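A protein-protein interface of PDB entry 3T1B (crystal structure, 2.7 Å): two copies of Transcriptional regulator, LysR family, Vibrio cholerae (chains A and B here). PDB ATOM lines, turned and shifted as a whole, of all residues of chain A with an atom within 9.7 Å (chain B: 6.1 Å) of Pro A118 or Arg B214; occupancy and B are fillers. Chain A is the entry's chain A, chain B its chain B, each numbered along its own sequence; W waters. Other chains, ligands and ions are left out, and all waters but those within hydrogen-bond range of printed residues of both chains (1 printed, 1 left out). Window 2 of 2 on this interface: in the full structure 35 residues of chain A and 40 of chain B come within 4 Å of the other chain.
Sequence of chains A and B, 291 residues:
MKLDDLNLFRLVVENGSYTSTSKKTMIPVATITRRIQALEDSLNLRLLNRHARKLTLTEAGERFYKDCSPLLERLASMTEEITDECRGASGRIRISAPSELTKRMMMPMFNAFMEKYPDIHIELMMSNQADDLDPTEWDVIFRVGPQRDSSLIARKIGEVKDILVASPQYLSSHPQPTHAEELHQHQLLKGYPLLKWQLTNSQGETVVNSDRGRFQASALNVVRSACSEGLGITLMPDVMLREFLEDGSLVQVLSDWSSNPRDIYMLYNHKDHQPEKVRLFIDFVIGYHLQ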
ATOM      1  N   ALA A  89     -18.227 -33.282   6.126  1.00  0.00           N
ATOM      2  CA  ALA A  89     -17.948 -31.865   5.942  1.00  0.00           C
ATOM      3  C   ALA A  89     -17.204 -31.603   4.641  1.00  0.00           C
ATOM      4  O   ALA A  89     -16.390 -30.682   4.556  1.00  0.00           O
ATOM      5  CB  ALA A  89     -17.169 -31.316   7.121  1.00  0.00           C
ATOM      6  N   SER A  90     -17.485 -32.413   3.624  1.00  0.00           N
ATOM      7  CA  SER A  90     -16.848 -32.240   2.321  1.00  0.00           C
ATOM      8  C   SER A  90     -17.808 -32.559   1.180  1.00  0.00           C
ATOM      9  O   SER A  90     -18.896 -33.093   1.401  1.00  0.00           O
ATOM     10  CB  SER A  90     -15.608 -33.121   2.209  1.00  0.00           C
ATOM     11  OG  SER A  90     -15.965 -34.490   2.198  1.00  0.00           O
ATOM     12  N   GLY A  91     -17.400 -32.222  -0.040  1.00  0.00           N
ATOM     13  CA  GLY A  91     -18.209 -32.489  -1.216  1.00  0.00           C
ATOM     14  C   GLY A  91     -18.545 -31.227  -1.984  1.00  0.00           C
ATOM     15  O   GLY A  91     -18.242 -30.120  -1.536  1.00  0.00           O
ATOM     16  N   ARG A  92     -19.175 -31.394  -3.142  1.00  0.00           N
ATOM     17  CA  ARG A  92     -19.507 -30.267  -4.004  1.00  0.00           C
ATOM     18  C   ARG A  92     -20.926 -29.770  -3.753  1.00  0.00           C
ATOM     19  O   ARG A  92     -21.836 -30.565  -3.520  1.00  0.00           O
ATOM     20  CB  ARG A  92     -19.342 -30.657  -5.473  1.00  0.00           C
ATOM     21  CG  ARG A  92     -19.585 -29.519  -6.454  1.00  0.00           C
ATOM     22  CD  ARG A  92     -19.211 -29.931  -7.865  1.00  0.00           C
ATOM     23  NE  ARG A  92     -17.865 -30.498  -7.909  1.00  0.00           N
ATOM     24  CZ  ARG A  92     -16.754 -29.781  -8.043  1.00  0.00           C
ATOM     25  NH1 ARG A  92     -15.575 -30.387  -8.068  1.00  0.00           N
ATOM     26  NH2 ARG A  92     -16.819 -28.460  -8.154  1.00  0.00           N
ATOM     27  N   ILE A  93     -21.108 -28.452  -3.803  1.00  0.00           N
ATOM     28  CA  ILE A  93     -22.426 -27.846  -3.640  1.00  0.00           C
ATOM     29  C   ILE A  93     -22.754 -26.922  -4.812  1.00  0.00           C
ATOM     30  O   ILE A  93     -21.889 -26.200  -5.308  1.00  0.00           O
ATOM     31  CB  ILE A  93     -22.528 -27.048  -2.322  1.00  0.00           C
ATOM     32  CG1 ILE A  93     -21.586 -25.843  -2.347  1.00  0.00           C
ATOM     33  CG2 ILE A  93     -22.223 -27.937  -1.131  1.00  0.00           C
ATOM     34  CD1 ILE A  93     -21.603 -25.036  -1.074  1.00  0.00           C
ATOM     35  N   ILE A  95     -24.535 -23.683  -6.294  1.00  0.00           N
ATOM     36  CA  ILE A  95     -25.013 -22.375  -5.859  1.00  0.00           C
ATOM     37  C   ILE A  95     -25.395 -21.479  -7.036  1.00  0.00           C
ATOM     38  O   ILE A  95     -24.670 -21.393  -8.027  1.00  0.00           O
ATOM     39  CB  ILE A  95     -23.958 -21.656  -5.003  1.00  0.00           C
ATOM     40  CG1 ILE A  95     -23.650 -22.471  -3.748  1.00  0.00           C
ATOM     41  CG2 ILE A  95     -24.444 -20.267  -4.618  1.00  0.00           C
ATOM     42  CD1 ILE A  95     -22.574 -21.864  -2.881  1.00  0.00           C
ATOM     43  N   MET A 107     -18.627 -12.586  -3.748  1.00  0.00           N
ATOM     44  CA  MET A 107     -17.410 -13.363  -4.012  1.00  0.00           C
ATOM     45  C   MET A 107     -16.404 -13.351  -2.859  1.00  0.00           C
ATOM     46  O   MET A 107     -15.823 -14.387  -2.532  1.00  0.00           O
ATOM     47  CB  MET A 107     -16.736 -12.942  -5.321  1.00  0.00           C
ATOM     48  CG  MET A 107     -17.267 -13.670  -6.539  1.00  0.00           C
ATOM     49  SD  MET A 107     -17.423 -15.450  -6.274  1.00  0.00           S
ATOM     50  CE  MET A 107     -15.712 -15.910  -6.005  1.00  0.00           C
ATOM     51  N   PHE A 110     -17.687 -15.939  -0.596  1.00  0.00           N
ATOM     52  CA  PHE A 110     -17.488 -17.267  -1.167  1.00  0.00           C
ATOM     53  C   PHE A 110     -16.018 -17.666  -1.080  1.00  0.00           C
ATOM     54  O   PHE A 110     -15.694 -18.790  -0.699  1.00  0.00           O
ATOM     55  CB  PHE A 110     -17.963 -17.312  -2.624  1.00  0.00           C
ATOM     56  CG  PHE A 110     -19.441 -17.104  -2.790  1.00  0.00           C
ATOM     57  CD1 PHE A 110     -20.275 -17.045  -1.686  1.00  0.00           C
ATOM     58  CD2 PHE A 110     -20.000 -16.976  -4.052  1.00  0.00           C
ATOM     59  CE1 PHE A 110     -21.633 -16.855  -1.834  1.00  0.00           C
ATOM     60  CE2 PHE A 110     -21.358 -16.786  -4.207  1.00  0.00           C
ATOM     61  CZ  PHE A 110     -22.176 -16.724  -3.097  1.00  0.00           C
ATOM     62  N   ASN A 111     -15.134 -16.737  -1.433  1.00  0.00           N
ATOM     63  CA  ASN A 111     -13.701 -16.968  -1.320  1.00  0.00           C
ATOM     64  C   ASN A 111     -13.300 -17.316   0.108  1.00  0.00           C
ATOM     65  O   ASN A 111     -12.558 -18.266   0.343  1.00  0.00           O
ATOM     66  CB  ASN A 111     -12.913 -15.747  -1.795  1.00  0.00           C
ATOM     67  CG  ASN A 111     -12.940 -15.582  -3.300  1.00  0.00           C
ATOM     68  OD1 ASN A 111     -13.140 -16.544  -4.038  1.00  0.00           O
ATOM     69  ND2 ASN A 111     -12.729 -14.355  -3.764  1.00  0.00           N
ATOM     70  N   ALA A 112     -13.800 -16.536   1.059  1.00  0.00           N
ATOM     71  CA  ALA A 112     -13.510 -16.761   2.470  1.00  0.00           C
ATOM     72  C   ALA A 112     -13.977 -18.143   2.916  1.00  0.00           C
ATOM     73  O   ALA A 112     -13.288 -18.825   3.675  1.00  0.00           O
ATOM     74  CB  ALA A 112     -14.156 -15.682   3.322  1.00  0.00           C
ATOM     75  N   PHE A 113     -15.152 -18.546   2.445  1.00  0.00           N
ATOM     76  CA  PHE A 113     -15.701 -19.852   2.777  1.00  0.00           C
ATOM     77  C   PHE A 113     -14.810 -20.976   2.262  1.00  0.00           C
ATOM     78  O   PHE A 113     -14.484 -21.911   2.993  1.00  0.00           O
ATOM     79  CB  PHE A 113     -17.122 -20.003   2.220  1.00  0.00           C
ATOM     80  CG  PHE A 113     -17.649 -21.405   2.283  1.00  0.00           C
ATOM     81  CD1 PHE A 113     -18.177 -21.907   3.460  1.00  0.00           C
ATOM     82  CD2 PHE A 113     -17.613 -22.223   1.168  1.00  0.00           C
ATOM     83  CE1 PHE A 113     -18.658 -23.198   3.525  1.00  0.00           C
ATOM     84  CE2 PHE A 113     -18.095 -23.515   1.225  1.00  0.00           C
ATOM     85  CZ  PHE A 113     -18.618 -24.002   2.408  1.00  0.00           C
ATOM     86  N   MET A 114     -14.413 -20.877   0.998  1.00  0.00           N
ATOM     87  CA  MET A 114     -13.589 -21.908   0.374  1.00  0.00           C
ATOM     88  C   MET A 114     -12.216 -22.034   1.030  1.00  0.00           C
ATOM     89  O   MET A 114     -11.640 -23.123   1.071  1.00  0.00           O
ATOM     90  CB  MET A 114     -13.457 -21.660  -1.132  1.00  0.00           C
ATOM     91  CG  MET A 114     -14.732 -21.952  -1.910  1.00  0.00           C
ATOM     92  SD  MET A 114     -14.550 -21.812  -3.699  1.00  0.00           S
ATOM     93  CE  MET A 114     -14.505 -20.035  -3.922  1.00  0.00           C
ATOM     94  N   GLU A 115     -11.690 -20.924   1.541  1.00  0.00           N
ATOM     95  CA  GLU A 115     -10.436 -20.969   2.283  1.00  0.00           C
ATOM     96  C   GLU A 115     -10.616 -21.733   3.590  1.00  0.00           C
ATOM     97  O   GLU A 115      -9.770 -22.537   3.974  1.00  0.00           O
ATOM     98  CB  GLU A 115      -9.911 -19.561   2.563  1.00  0.00           C
ATOM     99  CG  GLU A 115      -8.791 -19.525   3.590  1.00  0.00           C
ATOM    100  CD  GLU A 115      -7.783 -18.424   3.324  1.00  0.00           C
ATOM    101  OE1 GLU A 115      -7.909 -17.735   2.286  1.00  0.00           O
ATOM    102  OE2 GLU A 115      -6.857 -18.251   4.149  1.00  0.00           O
ATOM    103  N   LYS A 116     -11.730 -21.474   4.265  1.00  0.00           N
ATOM    104  CA  LYS A 116     -12.029 -22.128   5.529  1.00  0.00           C
ATOM    105  C   LYS A 116     -12.301 -23.616   5.327  1.00  0.00           C
ATOM    106  O   LYS A 116     -11.896 -24.446   6.143  1.00  0.00           O
ATOM    107  CB  LYS A 116     -13.227 -21.455   6.197  1.00  0.00           C
ATOM    108  CG  LYS A 116     -13.685 -22.109   7.490  1.00  0.00           C
ATOM    109  CD  LYS A 116     -13.264 -21.303   8.703  1.00  0.00           C
ATOM    110  CE  LYS A 116     -13.944 -21.812   9.963  1.00  0.00           C
ATOM    111  NZ  LYS A 116     -15.430 -21.685   9.896  1.00  0.00           N
ATOM    112  N   TYR A 117     -12.984 -23.951   4.237  1.00  0.00           N
ATOM    113  CA  TYR A 117     -13.336 -25.338   3.947  1.00  0.00           C
ATOM    114  C   TYR A 117     -12.816 -25.777   2.581  1.00  0.00           C
ATOM    115  O   TYR A 117     -13.546 -25.727   1.591  1.00  0.00           O
ATOM    116  CB  TYR A 117     -14.855 -25.527   4.013  1.00  0.00           C
ATOM    117  CG  TYR A 117     -15.482 -25.079   5.316  1.00  0.00           C
ATOM    118  CD1 TYR A 117     -15.562 -25.937   6.404  1.00  0.00           C
ATOM    119  CD2 TYR A 117     -16.005 -23.802   5.454  1.00  0.00           C
ATOM    120  CE1 TYR A 117     -16.141 -25.531   7.595  1.00  0.00           C
ATOM    121  CE2 TYR A 117     -16.586 -23.390   6.640  1.00  0.00           C
ATOM    122  CZ  TYR A 117     -16.651 -24.258   7.708  1.00  0.00           C
ATOM    123  OH  TYR A 117     -17.232 -23.843   8.886  1.00  0.00           O
ATOM    124  N   PRO A 118     -11.551 -26.217   2.526  1.00  0.00           N
ATOM    125  CA  PRO A 118     -10.903 -26.617   1.272  1.00  0.00           C
ATOM    126  C   PRO A 118     -11.477 -27.898   0.668  1.00  0.00           C
ATOM    127  O   PRO A 118     -11.266 -28.156  -0.518  1.00  0.00           O
ATOM    128  CB  PRO A 118      -9.444 -26.840   1.686  1.00  0.00           C
ATOM    129  CG  PRO A 118      -9.507 -27.143   3.147  1.00  0.00           C
ATOM    130  CD  PRO A 118     -10.635 -26.305   3.675  1.00  0.00           C
ATOM    131  N   ASP A 119     -12.188 -28.685   1.466  1.00  0.00           N
ATOM    132  CA  ASP A 119     -12.736 -29.953   0.988  1.00  0.00           C
ATOM    133  C   ASP A 119     -14.163 -29.816   0.462  1.00  0.00           C
ATOM    134  O   ASP A 119     -14.736 -30.777  -0.055  1.00  0.00           O
ATOM    135  CB  ASP A 119     -12.675 -31.016   2.086  1.00  0.00           C
ATOM    136  CG  ASP A 119     -11.255 -31.398   2.447  1.00  0.00           C
ATOM    137  OD1 ASP A 119     -10.364 -31.265   1.581  1.00  0.00           O
ATOM    138  OD2 ASP A 119     -11.032 -31.833   3.594  1.00  0.00           O
ATOM    139  N   ILE A 120     -14.733 -28.624   0.599  1.00  0.00           N
ATOM    140  CA  ILE A 120     -16.052 -28.337   0.046  1.00  0.00           C
ATOM    141  C   ILE A 120     -15.918 -27.524  -1.236  1.00  0.00           C
ATOM    142  O   ILE A 120     -15.416 -26.400  -1.221  1.00  0.00           O
ATOM    143  CB  ILE A 120     -16.929 -27.563   1.042  1.00  0.00           C
ATOM    144  CG1 ILE A 120     -17.147 -28.390   2.311  1.00  0.00           C
ATOM    145  CG2 ILE A 120     -18.258 -27.212   0.406  1.00  0.00           C
ATOM    146  CD1 ILE A 120     -17.935 -27.664   3.386  1.00  0.00           C
ATOM    147  N   HIS A 121     -16.367 -28.096  -2.347  1.00  0.00           N
ATOM    148  CA  HIS A 121     -16.205 -27.461  -3.646  1.00  0.00           C
ATOM    149  C   HIS A 121     -17.477 -26.739  -4.074  1.00  0.00           C
ATOM    150  O   HIS A 121     -18.582 -27.168  -3.746  1.00  0.00           O
ATOM    151  CB  HIS A 121     -15.802 -28.500  -4.690  1.00  0.00           C
ATOM    152  CG  HIS A 121     -14.541 -29.231  -4.343  1.00  0.00           C
ATOM    153  ND1 HIS A 121     -13.744 -28.871  -3.283  1.00  0.00           N
ATOM    154  CD2 HIS A 121     -13.942 -30.299  -4.923  1.00  0.00           C
ATOM    155  CE1 HIS A 121     -12.703 -29.683  -3.218  1.00  0.00           C
ATOM    156  NE2 HIS A 121     -12.800 -30.559  -4.200  1.00  0.00           N
ATOM    157  N   ILE A 122     -17.316 -25.644  -4.811  1.00  0.00           N
ATOM    158  CA  ILE A 122     -18.451 -24.823  -5.228  1.00  0.00           C
ATOM    159  C   ILE A 122     -18.684 -24.825  -6.736  1.00  0.00           C
ATOM    160  O   ILE A 122     -17.792 -24.486  -7.515  1.00  0.00           O
ATOM    161  CB  ILE A 122     -18.284 -23.361  -4.769  1.00  0.00           C
ATOM    162  CG1 ILE A 122     -18.409 -23.259  -3.250  1.00  0.00           C
ATOM    163  CG2 ILE A 122     -19.309 -22.456  -5.447  1.00  0.00           C
ATOM    164  CD1 ILE A 122     -18.347 -21.846  -2.734  1.00  0.00           C
ATOM    165  N   GLU A 123     -19.893 -25.204  -7.140  1.00  0.00           N
ATOM    166  CA  GLU A 123     -20.335 -25.001  -8.514  1.00  0.00           C
ATOM    167  C   GLU A 123     -21.276 -23.803  -8.534  1.00  0.00           C
ATOM    168  O   GLU A 123     -22.359 -23.844  -7.949  1.00  0.00           O
ATOM    169  CB  GLU A 123     -21.026 -26.247  -9.071  1.00  0.00           C
ATOM    170  CG  GLU A 123     -21.544 -26.074 -10.490  1.00  0.00           C
ATOM    171  CD  GLU A 123     -21.963 -27.383 -11.130  1.00  0.00           C
ATOM    172  OE1 GLU A 123     -21.296 -28.413 -10.891  1.00  0.00           O
ATOM    173  OE2 GLU A 123     -22.967 -27.384 -11.873  1.00  0.00           O
ATOM    174  N   LEU A 124     -20.850 -22.731  -9.195  1.00  0.00           N
ATOM    175  CA  LEU A 124     -21.589 -21.475  -9.179  1.00  0.00           C
ATOM    176  C   LEU A 124     -22.155 -21.117 -10.552  1.00  0.00           C
ATOM    177  O   LEU A 124     -21.434 -21.100 -11.550  1.00  0.00           O
ATOM    178  CB  LEU A 124     -20.689 -20.344  -8.671  1.00  0.00           C
ATOM    179  CG  LEU A 124     -21.283 -18.935  -8.586  1.00  0.00           C
ATOM    180  CD1 LEU A 124     -22.391 -18.868  -7.540  1.00  0.00           C
ATOM    181  CD2 LEU A 124     -20.190 -17.931  -8.275  1.00  0.00           C
ATOM    182  N   LEU A 280     -22.938 -26.106   6.496  1.00  0.00           N
ATOM    183  CA  LEU A 280     -21.753 -25.334   6.844  1.00  0.00           C
ATOM    184  C   LEU A 280     -21.678 -24.051   6.024  1.00  0.00           C
ATOM    185  O   LEU A 280     -21.213 -23.019   6.510  1.00  0.00           O
ATOM    186  CB  LEU A 280     -20.485 -26.166   6.654  1.00  0.00           C
ATOM    187  CG  LEU A 280     -20.200 -27.213   7.734  1.00  0.00           C
ATOM    188  CD1 LEU A 280     -19.003 -28.073   7.350  1.00  0.00           C
ATOM    189  CD2 LEU A 280     -19.981 -26.548   9.086  1.00  0.00           C
ATOM    190  N   TYR B 170      -0.653 -18.870  -3.005  1.00  0.00           N
ATOM    191  CA  TYR B 170      -0.976 -20.267  -3.266  1.00  0.00           C
ATOM    192  C   TYR B 170       0.268 -21.064  -3.631  1.00  0.00           C
ATOM    193  O   TYR B 170       0.441 -22.200  -3.190  1.00  0.00           O
ATOM    194  CB  TYR B 170      -2.013 -20.383  -4.385  1.00  0.00           C
ATOM    195  CG  TYR B 170      -2.236 -21.803  -4.858  1.00  0.00           C
ATOM    196  CD1 TYR B 170      -3.160 -22.626  -4.229  1.00  0.00           C
ATOM    197  CD2 TYR B 170      -1.520 -22.320  -5.930  1.00  0.00           C
ATOM    198  CE1 TYR B 170      -3.365 -23.925  -4.654  1.00  0.00           C
ATOM    199  CE2 TYR B 170      -1.719 -23.619  -6.363  1.00  0.00           C
ATOM    200  CZ  TYR B 170      -2.644 -24.415  -5.719  1.00  0.00           C
ATOM    201  OH  TYR B 170      -2.849 -25.710  -6.141  1.00  0.00           O
ATOM    202  N   GLN B 187      -5.346 -27.511  -6.625  1.00  0.00           N
ATOM    203  CA  GLN B 187      -6.657 -26.883  -6.568  1.00  0.00           C
ATOM    204  C   GLN B 187      -6.875 -26.057  -7.833  1.00  0.00           C
ATOM    205  O   GLN B 187      -6.174 -25.072  -8.069  1.00  0.00           O
ATOM    206  CB  GLN B 187      -6.758 -25.987  -5.335  1.00  0.00           C
ATOM    207  CG  GLN B 187      -6.509 -26.715  -4.029  1.00  0.00           C
ATOM    208  CD  GLN B 187      -7.439 -27.897  -3.848  1.00  0.00           C
ATOM    209  OE1 GLN B 187      -8.634 -27.727  -3.599  1.00  0.00           O
ATOM    210  NE2 GLN B 187      -6.898 -29.106  -3.983  1.00  0.00           N
ATOM    211  N   LEU B 188      -7.839 -26.465  -8.651  1.00  0.00           N
ATOM    212  CA  LEU B 188      -8.081 -25.797  -9.922  1.00  0.00           C
ATOM    213  C   LEU B 188      -9.328 -24.927  -9.862  1.00  0.00           C
ATOM    214  O   LEU B 188     -10.308 -25.273  -9.201  1.00  0.00           O
ATOM    215  CB  LEU B 188      -8.208 -26.821 -11.053  1.00  0.00           C
ATOM    216  CG  LEU B 188      -7.035 -27.790 -11.222  1.00  0.00           C
ATOM    217  CD1 LEU B 188      -7.239 -28.670 -12.444  1.00  0.00           C
ATOM    218  CD2 LEU B 188      -5.717 -27.029 -11.323  1.00  0.00           C
ATOM    219  N   LEU B 189      -9.285 -23.794 -10.555  1.00  0.00           N
ATOM    220  CA  LEU B 189     -10.423 -22.887 -10.616  1.00  0.00           C
ATOM    221  C   LEU B 189     -10.833 -22.691 -12.069  1.00  0.00           C
ATOM    222  O   LEU B 189     -10.078 -22.136 -12.866  1.00  0.00           O
ATOM    223  CB  LEU B 189     -10.062 -21.544  -9.983  1.00  0.00           C
ATOM    224  CG  LEU B 189      -9.270 -21.636  -8.678  1.00  0.00           C
ATOM    225  CD1 LEU B 189      -8.883 -20.259  -8.184  1.00  0.00           C
ATOM    226  CD2 LEU B 189     -10.057 -22.387  -7.619  1.00  0.00           C
ATOM    227  N   ARG B 212     -13.605 -31.061 -12.371  1.00  0.00           N
ATOM    228  CA  ARG B 212     -14.664 -30.095 -12.112  1.00  0.00           C
ATOM    229  C   ARG B 212     -14.098 -28.897 -11.359  1.00  0.00           C
ATOM    230  O   ARG B 212     -14.639 -27.794 -11.426  1.00  0.00           O
ATOM    231  CB  ARG B 212     -15.802 -30.742 -11.320  1.00  0.00           C
ATOM    232  CG  ARG B 212     -16.413 -31.956 -12.003  1.00  0.00           C
ATOM    233  CD  ARG B 212     -17.486 -32.610 -11.145  1.00  0.00           C
ATOM    234  NE  ARG B 212     -18.672 -31.768 -11.001  1.00  0.00           N
ATOM    235  CZ  ARG B 212     -19.718 -31.802 -11.820  1.00  0.00           C
ATOM    236  NH1 ARG B 212     -19.729 -32.637 -12.851  1.00  0.00           N
ATOM    237  NH2 ARG B 212     -20.755 -30.998 -11.611  1.00  0.00           N
ATOM    238  N   GLY B 213     -13.003 -29.126 -10.640  1.00  0.00           N
ATOM    239  CA  GLY B 213     -12.296 -28.061  -9.949  1.00  0.00           C
ATOM    240  C   GLY B 213     -12.841 -27.730  -8.574  1.00  0.00           C
ATOM    241  O   GLY B 213     -13.998 -28.018  -8.260  1.00  0.00           O
ATOM    242  N   ARG B 214     -11.991 -27.126  -7.748  1.00  0.00           N
ATOM    243  CA  ARG B 214     -12.394 -26.643  -6.436  1.00  0.00           C
ATOM    244  C   ARG B 214     -13.490 -25.602  -6.600  1.00  0.00           C
ATOM    245  O   ARG B 214     -14.375 -25.468  -5.754  1.00  0.00           O
ATOM    246  CB  ARG B 214     -11.195 -26.020  -5.725  1.00  0.00           C
ATOM    247  CG  ARG B 214     -11.501 -25.398  -4.374  1.00  0.00           C
ATOM    248  CD  ARG B 214     -10.260 -24.721  -3.819  1.00  0.00           C
ATOM    249  NE  ARG B 214     -10.393 -24.365  -2.410  1.00  0.00           N
ATOM    250  CZ  ARG B 214      -9.397 -23.902  -1.662  1.00  0.00           C
ATOM    251  NH1 ARG B 214      -8.192 -23.738  -2.188  1.00  0.00           N
ATOM    252  NH2 ARG B 214      -9.605 -23.607  -0.385  1.00  0.00           N
ATOM    253  N   PHE B 215     -13.425 -24.869  -7.706  1.00  0.00           N
ATOM    254  CA  PHE B 215     -14.372 -23.800  -7.975  1.00  0.00           C
ATOM    255  C   PHE B 215     -14.714 -23.726  -9.461  1.00  0.00           C
ATOM    256  O   PHE B 215     -13.845 -23.484 -10.300  1.00  0.00           O
ATOM    257  CB  PHE B 215     -13.806 -22.465  -7.487  1.00  0.00           C
ATOM    258  CG  PHE B 215     -14.725 -21.299  -7.703  1.00  0.00           C
ATOM    259  CD1 PHE B 215     -16.051 -21.358  -7.302  1.00  0.00           C
ATOM    260  CD2 PHE B 215     -14.260 -20.136  -8.292  1.00  0.00           C
ATOM    261  CE1 PHE B 215     -16.896 -20.279  -7.497  1.00  0.00           C
ATOM    262  CE2 PHE B 215     -15.097 -19.055  -8.489  1.00  0.00           C
ATOM    263  CZ  PHE B 215     -16.419 -19.125  -8.090  1.00  0.00           C
ATOM    264  N   GLN B 216     -15.987 -23.950  -9.774  1.00  0.00           N
ATOM    265  CA  GLN B 216     -16.471 -23.857 -11.145  1.00  0.00           C
ATOM    266  C   GLN B 216     -17.557 -22.795 -11.254  1.00  0.00           C
ATOM    267  O   GLN B 216     -18.546 -22.828 -10.520  1.00  0.00           O
ATOM    268  CB  GLN B 216     -17.011 -25.202 -11.633  1.00  0.00           C
ATOM    269  CG  GLN B 216     -17.689 -25.131 -12.997  1.00  0.00           C
ATOM    270  CD  GLN B 216     -18.424 -26.408 -13.362  1.00  0.00           C
ATOM    271  OE1 GLN B 216     -17.995 -27.510 -13.018  1.00  0.00           O
ATOM    272  NE2 GLN B 216     -19.545 -26.262 -14.056  1.00  0.00           N
ATOM    273  N   GLY B 230      -5.862 -16.712  -3.861  1.00  0.00           N
ATOM    274  CA  GLY B 230      -4.966 -17.839  -3.672  1.00  0.00           C
ATOM    275  C   GLY B 230      -5.655 -19.172  -3.461  1.00  0.00           C
ATOM    276  O   GLY B 230      -5.185 -20.004  -2.685  1.00  0.00           O
ATOM    277  N   LEU B 231      -6.766 -19.380  -4.157  1.00  0.00           N
ATOM    278  CA  LEU B 231      -7.531 -20.613  -4.008  1.00  0.00           C
ATOM    279  C   LEU B 231      -7.165 -21.675  -5.046  1.00  0.00           C
ATOM    280  O   LEU B 231      -7.727 -22.769  -5.043  1.00  0.00           O
ATOM    281  CB  LEU B 231      -9.034 -20.321  -4.034  1.00  0.00           C
ATOM    282  CG  LEU B 231      -9.547 -19.451  -2.887  1.00  0.00           C
ATOM    283  CD1 LEU B 231     -11.045 -19.195  -3.032  1.00  0.00           C
ATOM    284  CD2 LEU B 231      -9.230 -20.076  -1.532  1.00  0.00           C
ATOM    285  N   GLY B 232      -6.226 -21.353  -5.931  1.00  0.00           N
ATOM    286  CA  GLY B 232      -5.744 -22.329  -6.890  1.00  0.00           C
ATOM    287  C   GLY B 232      -5.323 -21.779  -8.241  1.00  0.00           C
ATOM    288  O   GLY B 232      -5.138 -20.572  -8.412  1.00  0.00           O
HETATM  289  O   HOH W   1      -7.570 -23.190   1.712  1.00  0.00           O
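O of Gly B213 is in hydrogen-bond range of NH1 of Arg A92, 2.9 Å away. O of Met A114 sits at hydrogen-bond distance from NH2 of Arg B214, 2.5 Å away. The backbone carbonyl oxygen (O) of Arg B214 sits at hydrogen-bond distance from the backbone NH (N) of Ile A122 (3.1 Å). The backbone carbonyl oxygen (O) of Ile A122 is in hydrogen-bond range of the backbone NH (N) of Gln B216, at 2.9 Å. The side-chain carboxylate (OE1) of Glu A123 lies within salt-bridge range of the guanidinium group (NH2) of Arg B212. The backbone NH (N) of Leu A124 is in hydrogen-bond range of the backbone carbonyl oxygen (O) of Gln B216 (2.7 Å). The guanidinium group (NE) of Arg A92 sits close to the guanidinium group (NE) of Arg B212 (3.4 Å).
O of Gly A91 is in hydrogen-bond range of N of His A121. The backbone carbonyl oxygen (O) of Ile A93 is in hydrogen-bond range of the backbone NH (N) of Glu A123, at 2.9 Å. The backbone carbonyl oxygen (O) of Glu A123 is in hydrogen-bond range of the backbone NH (N) of Ile A95, at 2.7 Å. The side-chain amide nitrogen of Asn A111 sits close to the backbone carbonyl oxygen of Met A107. The backbone NH (N) of Arg B214 lies within hydrogen-bond range of the backbone carbonyl oxygen (O) of Leu B188 (2.9 Å). The guanidinium group (NH1) of Arg B214 is in hydrogen-bond range of the backbone carbonyl oxygen (O) of Leu B231 (3.1 Å).
Among the printed residues, pairs that only touch across the chains: His A121 with Arg B214 (3.4 Å), Glu A123 with Gln B216 (3.5 Å), Ile A122 with Phe B215 (3.5 Å), Asn A111 with Leu B231 (3.5 Å), Met A114 with Leu B231 (3.7 Å), Pro A118 with Arg B214 (3.7 Å), Glu A115 with Arg B214 (3.8 Å), Met A107 with Phe B215 (3.9 Å), Met A114 with Phe B215 (3.9 Å) and Leu A124 with Phe B215 (3.96 Å).
Printed residues of chain B within 4 Å of Glu A115: Arg B214 (3.8 Å). Tyr A117 touches none of the printed residues of chain B. Pro A118 touches one residue of chain B. Of the printed residues of chain B, His A121 touches Arg B214 (3.4 Å). Printed residues of chain B within 4 Å of Leu A124: Phe B215 (3.96 Å) and Gln B216 (2.7 Å). Arg B214 touches five residues of chain A. Leu B231 touches just these residues of chain A: Asn A111 (3.5 Å) and Met A114 (3.7 Å).
Of the 23 printed residues of chain A, 10 touch a printed residue of chain B. Printed residues of chain A that touch a printed residue of chain B: Arg A92, Met A107, Asn A111, Met A114, Glu A115, Pro A118, His A121, Ile A122, Glu A123 and Leu A124. Along chain A the printed residues that touch a printed residue of chain B span positions 92 to 124. Of the 12 printed residues of chain B, 6 touch a printed residue of chain A. Hydrophobic or aromatic side chains of chain B within 4 Å of the printed part of chain A: Phe B215 and Leu B231. Along chain B the printed residues that touch a printed residue of chain A span positions 212 to 231. Among the printed residues, Asp or Glu carboxylates within 4 Å of a Lys or Arg side-chain nitrogen of the other chain: Glu A123 with Arg B212 (2.7 Å).
No position is printed for both chains.
Water W1 lies within hydrogen-bond range of the guanidinium group (NH2) of Arg B214 and the backbone carbonyl oxygen (O) of Glu A115.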
